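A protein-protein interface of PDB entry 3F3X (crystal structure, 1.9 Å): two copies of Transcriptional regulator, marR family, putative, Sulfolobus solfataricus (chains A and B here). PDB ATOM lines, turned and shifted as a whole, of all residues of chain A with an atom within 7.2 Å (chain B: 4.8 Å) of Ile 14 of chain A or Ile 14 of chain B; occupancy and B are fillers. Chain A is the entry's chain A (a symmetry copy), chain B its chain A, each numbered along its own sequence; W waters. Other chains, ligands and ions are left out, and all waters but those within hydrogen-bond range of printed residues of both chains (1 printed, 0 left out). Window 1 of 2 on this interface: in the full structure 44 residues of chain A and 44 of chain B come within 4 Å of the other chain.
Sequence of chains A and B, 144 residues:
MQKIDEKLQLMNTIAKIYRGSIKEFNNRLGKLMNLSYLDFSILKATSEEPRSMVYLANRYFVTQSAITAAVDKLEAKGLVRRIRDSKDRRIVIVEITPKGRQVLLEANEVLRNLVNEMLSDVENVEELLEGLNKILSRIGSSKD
Leu 10 of chain A touches Leu 132 of chain B, and with the chains exchanged Leu 132 of chain A touches Leu 10 of chain B.
Ile 14 of chain A touches Leu 132 of chain B, and with the chains exchanged Leu 132 of chain A touches Ile 14 of chain B.
Ala 15 of chain A touches Tyr 18 of chain B, and with the chains exchanged Tyr 18 of chain A touches Ala 15 of chain B.
Tyr 18 of chain B touches its own counterpart, Tyr 18 of chain A.
10 positions are printed for both chains.
The side-chain hydroxyl (OH) of Tyr 37 of chain A sits close to the side-chain amide oxygen (OD1) of Asn 12 of chain B, 2.3 Å away.
Water W1 lies within hydrogen-bond range of O of Met 11 of chain B (3.0 Å), OG of Ser 21 of chain A (3.0 Å) and N of Ala 15 of chain B (3.4 Å).
Of the 20 printed residues of chain A, 13 touch a printed residue of chain B.
Printed residues of chain A that touch a printed residue of chain B: Leu 10, Met 11, Thr 13, Ile 14, Ala 15, Ile 17, Tyr 18, Arg 19, Ser 21, Tyr 37, Leu 132, Ile 135 and Leu 136.
Hydrophobic or aromatic side chains of chain A that line the printed part of chain B: Leu 10, Met 11, Ile 14, Ala 15, Ile 17, Tyr 18, Tyr 37, Leu 132, Ile 135 and Leu 136.
Of the 10 printed residues of chain B, 10 touch a printed residue of chain A.
Hydrophobic or aromatic side chains of chain B that line the printed part of chain A: Leu 10, Met 11, Ile 14, Ala 15, Ile 17, Tyr 18 and Leu 132.
Among the printed residues, no Asp or Glu carboxylate lies within 4 Å of a Lys or Arg side-chain nitrogen of the other chain.
Among the printed residues, merely in contact across the chains: Leu 10 of chain A with Leu 132 of chain B (3.2 Å), Met 11 of chain A with Ile 17 of chain B (3.7 Å), Thr 13 of chain A with Leu 132 of chain B (3.7 Å), Ile 14 of chain A with Ile 14 of chain B (3.9 Å), Ile 14 of chain A with Ile 17 of chain B (3.9 Å), Ile 14 of chain A with Leu 132 of chain B (3.6 Å), Ala 15 of chain A with Tyr 18 of chain B (3.5 Å), Ile 17 of chain A with Met 11 of chain B (3.7 Å), Ile 17 of chain A with Ile 14 of chain B (3.9 Å), Ile 17 of chain A with Leu 132 of chain B (3.5 Å), Tyr 18 of chain A with Ala 15 of chain B (3.5 Å), Tyr 18 of chain A with Tyr 18 of chain B (3.0 Å), Arg 19 of chain A with Tyr 18 of chain B (3.5 Å), Ser 21 of chain A with Met 11 of chain B (3.3 Å), Tyr 37 of chain A with Met 11 of chain B (3.8 Å), Tyr 37 of chain A with Ala 15 of chain B (3.8 Å), Leu 132 of chain A with Leu 10 of chain B (3.2 Å), Leu 132 of chain A with Thr 13 of chain B (3.7 Å), Leu 132 of chain A with Ile 14 of chain B (3.6 Å), Leu 132 of chain A with Ile 17 of chain B (3.5 Å), Ile 135 of chain A with Ile 17 of chain B (3.95 Å), Leu 136 of chain A with Lys 16 of chain B (3.4 Å) and Leu 136 of chain A with Ile 17 of chain B (3.8 Å).
Ile 14 of chain B touches just these residues of chain A: Ile 14 (3.9 Å), Ile 17 (3.9 Å) and Leu 132 (3.6 Å).
Of the printed residues of chain A, Ile 17 of chain B touches Met 11, Ile 14, Leu 132, Ile 135 and Leu 136.
Printed residues of chain A within 4 Å of Asn 12 of chain B: Tyr 37 (2.3 Å).
The nearest residue of chain B that does not touch Ile 14 of chain A is Tyr 18 of chain B (4.2 Å).
The nearest residue of chain A that does not touch Ile 14 of chain B is Tyr 18 of chain A (4.2 Å).
The nearest printed residue of chain B that does not touch Leu 132 of chain A is Leu 132 of chain B (4.3 Å).
The side-chain hydroxyl (OG1) of Thr 13 of chain A sits at hydrogen-bond distance from the backbone carbonyl oxygen (O) of Gln 9 of chain A (3.0 Å).
OG of Ser 21 of chain A sits at hydrogen-bond distance from O of Ile 17 of chain A (2.8 Å).
The side-chain hydroxyl of Ser 21 of chain A sits at hydrogen-bond distance from the backbone carbonyl oxygen of Tyr 18 of chain A, at 3.3 Å.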
ATOM      1  N   LYS A   7     -30.891 -13.137  15.495  1.00  0.00           N
ATOM      2  CA  LYS A   7     -30.704 -12.127  16.528  1.00  0.00           C
ATOM      3  C   LYS A   7     -29.964 -12.674  17.739  1.00  0.00           C
ATOM      4  O   LYS A   7     -29.106 -11.994  18.304  1.00  0.00           O
ATOM      5  CB  LYS A   7     -32.053 -11.520  16.927  1.00  0.00           C
ATOM      6  CG  LYS A   7     -32.686 -10.720  15.784  1.00  0.00           C
ATOM      7  CD  LYS A   7     -34.036 -10.124  16.157  1.00  0.00           C
ATOM      8  CE  LYS A   7     -34.668  -9.435  14.955  1.00  0.00           C
ATOM      9  NZ  LYS A   7     -36.020  -8.879  15.261  1.00  0.00           N
ATOM     10  N   LEU A   8     -30.278 -13.904  18.138  1.00  0.00           N
ATOM     11  CA  LEU A   8     -29.579 -14.494  19.273  1.00  0.00           C
ATOM     12  C   LEU A   8     -28.112 -14.704  18.908  1.00  0.00           C
ATOM     13  O   LEU A   8     -27.225 -14.514  19.741  1.00  0.00           O
ATOM     14  CB  LEU A   8     -30.196 -15.838  19.668  1.00  0.00           C
ATOM     15  CG  LEU A   8     -29.432 -16.579  20.777  1.00  0.00           C
ATOM     16  CD1 LEU A   8     -29.239 -15.666  21.989  1.00  0.00           C
ATOM     17  CD2 LEU A   8     -30.186 -17.842  21.165  1.00  0.00           C
ATOM     18  N   GLN A   9     -27.855 -15.096  17.662  1.00  0.00           N
ATOM     19  CA  GLN A   9     -26.478 -15.329  17.234  1.00  0.00           C
ATOM     20  C   GLN A   9     -25.718 -14.013  17.250  1.00  0.00           C
ATOM     21  O   GLN A   9     -24.518 -13.973  17.534  1.00  0.00           O
ATOM     22  CB  GLN A   9     -26.445 -15.948  15.835  1.00  0.00           C
ATOM     23  CG  GLN A   9     -25.094 -16.549  15.446  1.00  0.00           C
ATOM     24  CD  GLN A   9     -24.523 -17.466  16.523  1.00  0.00           C
ATOM     25  OE1 GLN A   9     -25.262 -18.182  17.197  1.00  0.00           O
ATOM     26  NE2 GLN A   9     -23.200 -17.454  16.677  1.00  0.00           N
ATOM     27  N   LEU A  10     -26.433 -12.932  16.955  1.00  0.00           N
ATOM     28  CA  LEU A  10     -25.840 -11.602  16.959  1.00  0.00           C
ATOM     29  C   LEU A  10     -25.309 -11.341  18.365  1.00  0.00           C
ATOM     30  O   LEU A  10     -24.185 -10.862  18.546  1.00  0.00           O
ATOM     31  CB  LEU A  10     -26.909 -10.568  16.599  1.00  0.00           C
ATOM     32  CG  LEU A  10     -26.453  -9.161  16.237  1.00  0.00           C
ATOM     33  CD1 LEU A  10     -25.615  -9.214  14.965  1.00  0.00           C
ATOM     34  CD2 LEU A  10     -27.674  -8.279  16.023  1.00  0.00           C
ATOM     35  N   MET A  11     -26.123 -11.674  19.362  1.00  0.00           N
ATOM     36  CA  MET A  11     -25.739 -11.481  20.753  1.00  0.00           C
ATOM     37  C   MET A  11     -24.621 -12.443  21.174  1.00  0.00           C
ATOM     38  O   MET A  11     -23.740 -12.069  21.954  1.00  0.00           O
ATOM     39  CB  MET A  11     -26.964 -11.639  21.662  1.00  0.00           C
ATOM     40  CG  MET A  11     -28.105 -10.667  21.335  1.00  0.00           C
ATOM     41  SD  MET A  11     -27.643  -8.899  21.406  1.00  0.00           S
ATOM     42  CE  MET A  11     -27.376  -8.716  23.107  1.00  0.00           C
ATOM     43  N   ASN A  12     -24.648 -13.675  20.660  1.00  0.00           N
ATOM     44  CA  ASN A  12     -23.605 -14.640  20.994  1.00  0.00           C
ATOM     45  C   ASN A  12     -22.255 -14.124  20.517  1.00  0.00           C
ATOM     46  O   ASN A  12     -21.246 -14.278  21.197  1.00  0.00           O
ATOM     47  CB  ASN A  12     -23.864 -15.993  20.325  1.00  0.00           C
ATOM     48  CG  ASN A  12     -25.020 -16.737  20.942  1.00  0.00           C
ATOM     49  OD1 ASN A  12     -25.272 -16.631  22.142  1.00  0.00           O
ATOM     50  ND2 ASN A  12     -25.713 -17.520  20.131  1.00  0.00           N
ATOM     51  N   THR A  13     -22.244 -13.519  19.336  1.00  0.00           N
ATOM     52  CA  THR A  13     -21.010 -12.990  18.766  1.00  0.00           C
ATOM     53  C   THR A  13     -20.537 -11.758  19.544  1.00  0.00           C
ATOM     54  O   THR A  13     -19.349 -11.606  19.821  1.00  0.00           O
ATOM     55  CB  THR A  13     -21.217 -12.623  17.289  1.00  0.00           C
ATOM     56  OG1 THR A  13     -21.695 -13.775  16.580  1.00  0.00           O
ATOM     57  CG2 THR A  13     -19.911 -12.153  16.661  1.00  0.00           C
ATOM     58  N   ILE A  14     -21.474 -10.887  19.904  1.00  0.00           N
ATOM     59  CA  ILE A  14     -21.142  -9.688  20.664  1.00  0.00           C
ATOM     60  C   ILE A  14     -20.506 -10.091  21.990  1.00  0.00           C
ATOM     61  O   ILE A  14     -19.563  -9.452  22.460  1.00  0.00           O
ATOM     62  CB  ILE A  14     -22.413  -8.826  20.899  1.00  0.00           C
ATOM     63  CG1 ILE A  14     -22.772  -8.111  19.592  1.00  0.00           C
ATOM     64  CG2 ILE A  14     -22.200  -7.832  22.047  1.00  0.00           C
ATOM     65  CD1 ILE A  14     -24.035  -7.281  19.661  1.00  0.00           C
ATOM     66  N   ALA A  15     -21.011 -11.167  22.581  1.00  0.00           N
ATOM     67  CA  ALA A  15     -20.484 -11.665  23.844  1.00  0.00           C
ATOM     68  C   ALA A  15     -19.011 -12.032  23.710  1.00  0.00           C
ATOM     69  O   ALA A  15     -18.200 -11.693  24.574  1.00  0.00           O
ATOM     70  CB  ALA A  15     -21.285 -12.884  24.306  1.00  0.00           C
ATOM     71  N   LYS A  16     -18.677 -12.723  22.622  1.00  0.00           N
ATOM     72  CA  LYS A  16     -17.305 -13.145  22.359  1.00  0.00           C
ATOM     73  C   LYS A  16     -16.393 -11.946  22.121  1.00  0.00           C
ATOM     74  O   LYS A  16     -15.278 -11.893  22.635  1.00  0.00           O
ATOM     75  CB  LYS A  16     -17.255 -14.054  21.127  1.00  0.00           C
ATOM     76  CG  LYS A  16     -18.115 -15.306  21.213  1.00  0.00           C
ATOM     77  CD  LYS A  16     -18.057 -16.071  19.896  1.00  0.00           C
ATOM     78  CE  LYS A  16     -18.967 -17.287  19.900  1.00  0.00           C
ATOM     79  NZ  LYS A  16     -18.860 -18.030  18.615  1.00  0.00           N
ATOM     80  N   ILE A  17     -16.873 -10.992  21.330  1.00  0.00           N
ATOM     81  CA  ILE A  17     -16.102  -9.796  21.010  1.00  0.00           C
ATOM     82  C   ILE A  17     -15.729  -9.052  22.290  1.00  0.00           C
ATOM     83  O   ILE A  17     -14.583  -8.632  22.461  1.00  0.00           O
ATOM     84  CB  ILE A  17     -16.889  -8.853  20.071  1.00  0.00           C
ATOM     85  CG1 ILE A  17     -17.149  -9.560  18.733  1.00  0.00           C
ATOM     86  CG2 ILE A  17     -16.100  -7.561  19.843  1.00  0.00           C
ATOM     87  CD1 ILE A  17     -18.011  -8.774  17.748  1.00  0.00           C
ATOM     88  N   TYR A  18     -16.688  -8.902  23.198  1.00  0.00           N
ATOM     89  CA  TYR A  18     -16.410  -8.211  24.452  1.00  0.00           C
ATOM     90  C   TYR A  18     -15.361  -8.941  25.280  1.00  0.00           C
ATOM     91  O   TYR A  18     -14.378  -8.344  25.711  1.00  0.00           O
ATOM     92  CB  TYR A  18     -17.671  -8.069  25.299  1.00  0.00           C
ATOM     93  CG  TYR A  18     -17.369  -7.501  26.664  1.00  0.00           C
ATOM     94  CD1 TYR A  18     -17.118  -6.140  26.833  1.00  0.00           C
ATOM     95  CD2 TYR A  18     -17.274  -8.332  27.779  1.00  0.00           C
ATOM     96  CE1 TYR A  18     -16.791  -5.618  28.080  1.00  0.00           C
ATOM     97  CE2 TYR A  18     -16.946  -7.822  29.032  1.00  0.00           C
ATOM     98  CZ  TYR A  18     -16.703  -6.466  29.173  1.00  0.00           C
ATOM     99  OH  TYR A  18     -16.397  -5.956  30.414  1.00  0.00           O
ATOM    100  N   ARG A  19     -15.586 -10.230  25.523  1.00  0.00           N
ATOM    101  CA  ARG A  19     -14.653 -11.023  26.313  1.00  0.00           C
ATOM    102  C   ARG A  19     -13.252 -10.972  25.726  1.00  0.00           C
ATOM    103  O   ARG A  19     -12.270 -10.820  26.451  1.00  0.00           O
ATOM    104  CB  ARG A  19     -15.121 -12.478  26.382  1.00  0.00           C
ATOM    105  CG  ARG A  19     -16.415 -12.670  27.145  1.00  0.00           C
ATOM    106  CD  ARG A  19     -16.856 -14.114  27.066  1.00  0.00           C
ATOM    107  NE  ARG A  19     -18.145 -14.327  27.710  1.00  0.00           N
ATOM    108  CZ  ARG A  19     -19.007 -15.264  27.335  1.00  0.00           C
ATOM    109  NH1 ARG A  19     -18.707 -16.065  26.320  1.00  0.00           N
ATOM    110  NH2 ARG A  19     -20.164 -15.400  27.969  1.00  0.00           N
ATOM    111  N   GLY A  20     -13.161 -11.100  24.409  1.00  0.00           N
ATOM    112  CA  GLY A  20     -11.859 -11.064  23.769  1.00  0.00           C
ATOM    113  C   GLY A  20     -11.223  -9.685  23.792  1.00  0.00           C
ATOM    114  O   GLY A  20     -10.056  -9.540  24.152  1.00  0.00           O
ATOM    115  N   SER A  21     -11.990  -8.667  23.416  1.00  0.00           N
ATOM    116  CA  SER A  21     -11.461  -7.309  23.379  1.00  0.00           C
ATOM    117  C   SER A  21     -11.137  -6.730  24.751  1.00  0.00           C
ATOM    118  O   SER A  21     -10.124  -6.046  24.906  1.00  0.00           O
ATOM    119  CB  SER A  21     -12.427  -6.378  22.648  1.00  0.00           C
ATOM    120  OG  SER A  21     -13.594  -6.151  23.414  1.00  0.00           O
ATOM    121  N   TYR A  37     -10.061  -0.624  31.347  1.00  0.00           N
ATOM    122  CA  TYR A  37     -10.938  -0.093  30.317  1.00  0.00           C
ATOM    123  C   TYR A  37     -12.025   0.764  30.959  1.00  0.00           C
ATOM    124  O   TYR A  37     -12.425   1.788  30.408  1.00  0.00           O
ATOM    125  CB  TYR A  37     -11.577  -1.234  29.536  1.00  0.00           C
ATOM    126  CG  TYR A  37     -12.455  -0.786  28.391  1.00  0.00           C
ATOM    127  CD1 TYR A  37     -12.014   0.170  27.476  1.00  0.00           C
ATOM    128  CD2 TYR A  37     -13.699  -1.373  28.182  1.00  0.00           C
ATOM    129  CE1 TYR A  37     -12.790   0.526  26.373  1.00  0.00           C
ATOM    130  CE2 TYR A  37     -14.482  -1.028  27.083  1.00  0.00           C
ATOM    131  CZ  TYR A  37     -14.020  -0.084  26.182  1.00  0.00           C
ATOM    132  OH  TYR A  37     -14.783   0.209  25.073  1.00  0.00           O
ATOM    133  N   LEU A 119      -8.883  -3.875  13.538  1.00  0.00           N
ATOM    134  CA  LEU A 119     -10.011  -3.837  12.612  1.00  0.00           C
ATOM    135  C   LEU A 119      -9.724  -3.025  11.369  1.00  0.00           C
ATOM    136  O   LEU A 119     -10.627  -2.441  10.767  1.00  0.00           O
ATOM    137  CB  LEU A 119     -11.229  -3.245  13.329  1.00  0.00           C
ATOM    138  CG  LEU A 119     -11.646  -3.873  14.664  1.00  0.00           C
ATOM    139  CD1 LEU A 119     -12.939  -3.228  15.176  1.00  0.00           C
ATOM    140  CD2 LEU A 119     -11.842  -5.374  14.467  1.00  0.00           C
ATOM    141  N   LEU A 132     -25.571  -1.160  16.081  1.00  0.00           N
ATOM    142  CA  LEU A 132     -25.204  -1.436  17.461  1.00  0.00           C
ATOM    143  C   LEU A 132     -25.809  -0.421  18.432  1.00  0.00           C
ATOM    144  O   LEU A 132     -26.263  -0.797  19.511  1.00  0.00           O
ATOM    145  CB  LEU A 132     -23.680  -1.481  17.608  1.00  0.00           C
ATOM    146  CG  LEU A 132     -23.028  -2.675  16.895  1.00  0.00           C
ATOM    147  CD1 LEU A 132     -21.518  -2.604  17.050  1.00  0.00           C
ATOM    148  CD2 LEU A 132     -23.561  -3.981  17.481  1.00  0.00           C
ATOM    149  N   ILE A 135     -29.398  -1.354  18.935  1.00  0.00           N
ATOM    150  CA  ILE A 135     -29.482  -2.553  19.761  1.00  0.00           C
ATOM    151  C   ILE A 135     -29.289  -2.199  21.238  1.00  0.00           C
ATOM    152  O   ILE A 135     -30.063  -2.634  22.098  1.00  0.00           O
ATOM    153  CB  ILE A 135     -28.427  -3.600  19.326  1.00  0.00           C
ATOM    154  CG1 ILE A 135     -28.863  -4.243  18.007  1.00  0.00           C
ATOM    155  CG2 ILE A 135     -28.243  -4.655  20.410  1.00  0.00           C
ATOM    156  CD1 ILE A 135     -27.818  -5.140  17.386  1.00  0.00           C
ATOM    157  N   LEU A 136     -28.270  -1.393  21.533  1.00  0.00           N
ATOM    158  CA  LEU A 136     -28.013  -1.007  22.918  1.00  0.00           C
ATOM    159  C   LEU A 136     -29.219  -0.317  23.561  1.00  0.00           C
ATOM    160  O   LEU A 136     -29.555  -0.588  24.715  1.00  0.00           O
ATOM    161  CB  LEU A 136     -26.789  -0.088  23.011  1.00  0.00           C
ATOM    162  CG  LEU A 136     -26.498   0.399  24.439  1.00  0.00           C
ATOM    163  CD1 LEU A 136     -26.208  -0.797  25.349  1.00  0.00           C
ATOM    164  CD2 LEU A 136     -25.320   1.355  24.430  1.00  0.00           C
ATOM    165  N   LEU B  10     -17.245   1.746  18.209  1.00  0.00           N
ATOM    166  CA  LEU B  10     -17.931   0.501  17.894  1.00  0.00           C
ATOM    167  C   LEU B  10     -17.698  -0.458  19.057  1.00  0.00           C
ATOM    168  O   LEU B  10     -18.624  -1.117  19.539  1.00  0.00           O
ATOM    169  CB  LEU B  10     -17.352  -0.086  16.604  1.00  0.00           C
ATOM    170  CG  LEU B  10     -18.119  -1.208  15.919  1.00  0.00           C
ATOM    171  CD1 LEU B  10     -19.473  -0.684  15.455  1.00  0.00           C
ATOM    172  CD2 LEU B  10     -17.316  -1.709  14.727  1.00  0.00           C
ATOM    173  N   MET B  11     -16.451  -0.520  19.515  1.00  0.00           N
ATOM    174  CA  MET B  11     -16.091  -1.392  20.624  1.00  0.00           C
ATOM    175  C   MET B  11     -16.690  -0.904  21.949  1.00  0.00           C
ATOM    176  O   MET B  11     -17.090  -1.718  22.788  1.00  0.00           O
ATOM    177  CB  MET B  11     -14.566  -1.509  20.727  1.00  0.00           C
ATOM    178  CG  MET B  11     -13.901  -2.047  19.452  1.00  0.00           C
ATOM    179  SD  MET B  11     -14.502  -3.687  18.914  1.00  0.00           S
ATOM    180  CE  MET B  11     -13.884  -4.679  20.192  1.00  0.00           C
ATOM    181  N   ASN B  12     -16.759   0.415  22.141  1.00  0.00           N
ATOM    182  CA  ASN B  12     -17.338   0.957  23.366  1.00  0.00           C
ATOM    183  C   ASN B  12     -18.799   0.541  23.472  1.00  0.00           C
ATOM    184  O   ASN B  12     -19.285   0.218  24.551  1.00  0.00           O
ATOM    185  CB  ASN B  12     -17.273   2.487  23.384  1.00  0.00           C
ATOM    186  CG  ASN B  12     -15.875   3.008  23.585  1.00  0.00           C
ATOM    187  OD1 ASN B  12     -15.062   2.390  24.271  1.00  0.00           O
ATOM    188  ND2 ASN B  12     -15.593   4.168  23.011  1.00  0.00           N
ATOM    189  N   THR B  13     -19.496   0.564  22.343  1.00  0.00           N
ATOM    190  CA  THR B  13     -20.908   0.197  22.317  1.00  0.00           C
ATOM    191  C   THR B  13     -21.082  -1.308  22.544  1.00  0.00           C
ATOM    192  O   THR B  13     -21.968  -1.735  23.280  1.00  0.00           O
ATOM    193  CB  THR B  13     -21.540   0.596  20.975  1.00  0.00           C
ATOM    194  OG1 THR B  13     -21.336   1.998  20.757  1.00  0.00           O
ATOM    195  CG2 THR B  13     -23.033   0.297  20.970  1.00  0.00           C
ATOM    196  N   ILE B  14     -20.225  -2.107  21.916  1.00  0.00           N
ATOM    197  CA  ILE B  14     -20.284  -3.555  22.074  1.00  0.00           C
ATOM    198  C   ILE B  14     -20.089  -3.911  23.544  1.00  0.00           C
ATOM    199  O   ILE B  14     -20.736  -4.819  24.067  1.00  0.00           O
ATOM    200  CB  ILE B  14     -19.206  -4.241  21.190  1.00  0.00           C
ATOM    201  CG1 ILE B  14     -19.669  -4.204  19.730  1.00  0.00           C
ATOM    202  CG2 ILE B  14     -18.937  -5.674  21.663  1.00  0.00           C
ATOM    203  CD1 ILE B  14     -18.679  -4.785  18.746  1.00  0.00           C
ATOM    204  N   ALA B  15     -19.208  -3.178  24.215  1.00  0.00           N
ATOM    205  CA  ALA B  15     -18.940  -3.406  25.627  1.00  0.00           C
ATOM    206  C   ALA B  15     -20.207  -3.228  26.456  1.00  0.00           C
ATOM    207  O   ALA B  15     -20.499  -4.041  27.336  1.00  0.00           O
ATOM    208  CB  ALA B  15     -17.855  -2.446  26.120  1.00  0.00           C
ATOM    209  N   LYS B  16     -20.951  -2.163  26.165  1.00  0.00           N
ATOM    210  CA  LYS B  16     -22.189  -1.862  26.875  1.00  0.00           C
ATOM    211  C   LYS B  16     -23.251  -2.924  26.610  1.00  0.00           C
ATOM    212  O   LYS B  16     -23.941  -3.366  27.527  1.00  0.00           O
ATOM    213  CB  LYS B  16     -22.736  -0.499  26.438  1.00  0.00           C
ATOM    214  CG  LYS B  16     -21.789   0.673  26.645  1.00  0.00           C
ATOM    215  CD  LYS B  16     -22.405   1.948  26.082  1.00  0.00           C
ATOM    216  CE  LYS B  16     -21.463   3.135  26.187  1.00  0.00           C
ATOM    217  NZ  LYS B  16     -22.108   4.369  25.663  1.00  0.00           N
ATOM    218  N   ILE B  17     -23.381  -3.321  25.348  1.00  0.00           N
ATOM    219  CA  ILE B  17     -24.365  -4.322  24.953  1.00  0.00           C
ATOM    220  C   ILE B  17     -24.130  -5.622  25.719  1.00  0.00           C
ATOM    221  O   ILE B  17     -25.072  -6.228  26.232  1.00  0.00           O
ATOM    222  CB  ILE B  17     -24.310  -4.598  23.433  1.00  0.00           C
ATOM    223  CG1 ILE B  17     -24.675  -3.319  22.666  1.00  0.00           C
ATOM    224  CG2 ILE B  17     -25.274  -5.729  23.068  1.00  0.00           C
ATOM    225  CD1 ILE B  17     -24.558  -3.425  21.147  1.00  0.00           C
ATOM    226  N   TYR B  18     -22.873  -6.044  25.813  1.00  0.00           N
ATOM    227  CA  TYR B  18     -22.563  -7.272  26.537  1.00  0.00           C
ATOM    228  C   TYR B  18     -22.927  -7.168  28.012  1.00  0.00           C
ATOM    229  O   TYR B  18     -23.623  -8.027  28.547  1.00  0.00           O
ATOM    230  CB  TYR B  18     -21.080  -7.617  26.436  1.00  0.00           C
ATOM    231  CG  TYR B  18     -20.717  -8.792  27.308  1.00  0.00           C
ATOM    232  CD1 TYR B  18     -21.032 -10.094  26.923  1.00  0.00           C
ATOM    233  CD2 TYR B  18     -20.111  -8.601  28.549  1.00  0.00           C
ATOM    234  CE1 TYR B  18     -20.744 -11.178  27.745  1.00  0.00           C
ATOM    235  CE2 TYR B  18     -19.819  -9.678  29.383  1.00  0.00           C
ATOM    236  CZ  TYR B  18     -20.141 -10.962  28.974  1.00  0.00           C
ATOM    237  OH  TYR B  18     -19.836 -12.029  29.788  1.00  0.00           O
ATOM    238  N   LEU B 132     -20.059  -8.244  12.519  1.00  0.00           N
ATOM    239  CA  LEU B 132     -19.625  -8.699  13.830  1.00  0.00           C
ATOM    240  C   LEU B 132     -18.757  -9.954  13.746  1.00  0.00           C
ATOM    241  O   LEU B 132     -17.767 -10.067  14.467  1.00  0.00           O
ATOM    242  CB  LEU B 132     -20.836  -8.939  14.737  1.00  0.00           C
ATOM    243  CG  LEU B 132     -21.588  -7.655  15.115  1.00  0.00           C
ATOM    244  CD1 LEU B 132     -22.799  -7.999  15.966  1.00  0.00           C
ATOM    245  CD2 LEU B 132     -20.654  -6.714  15.875  1.00  0.00           C
HETATM  246  O   HOH W   1     -16.087  -4.418  23.506  1.00  0.00           O
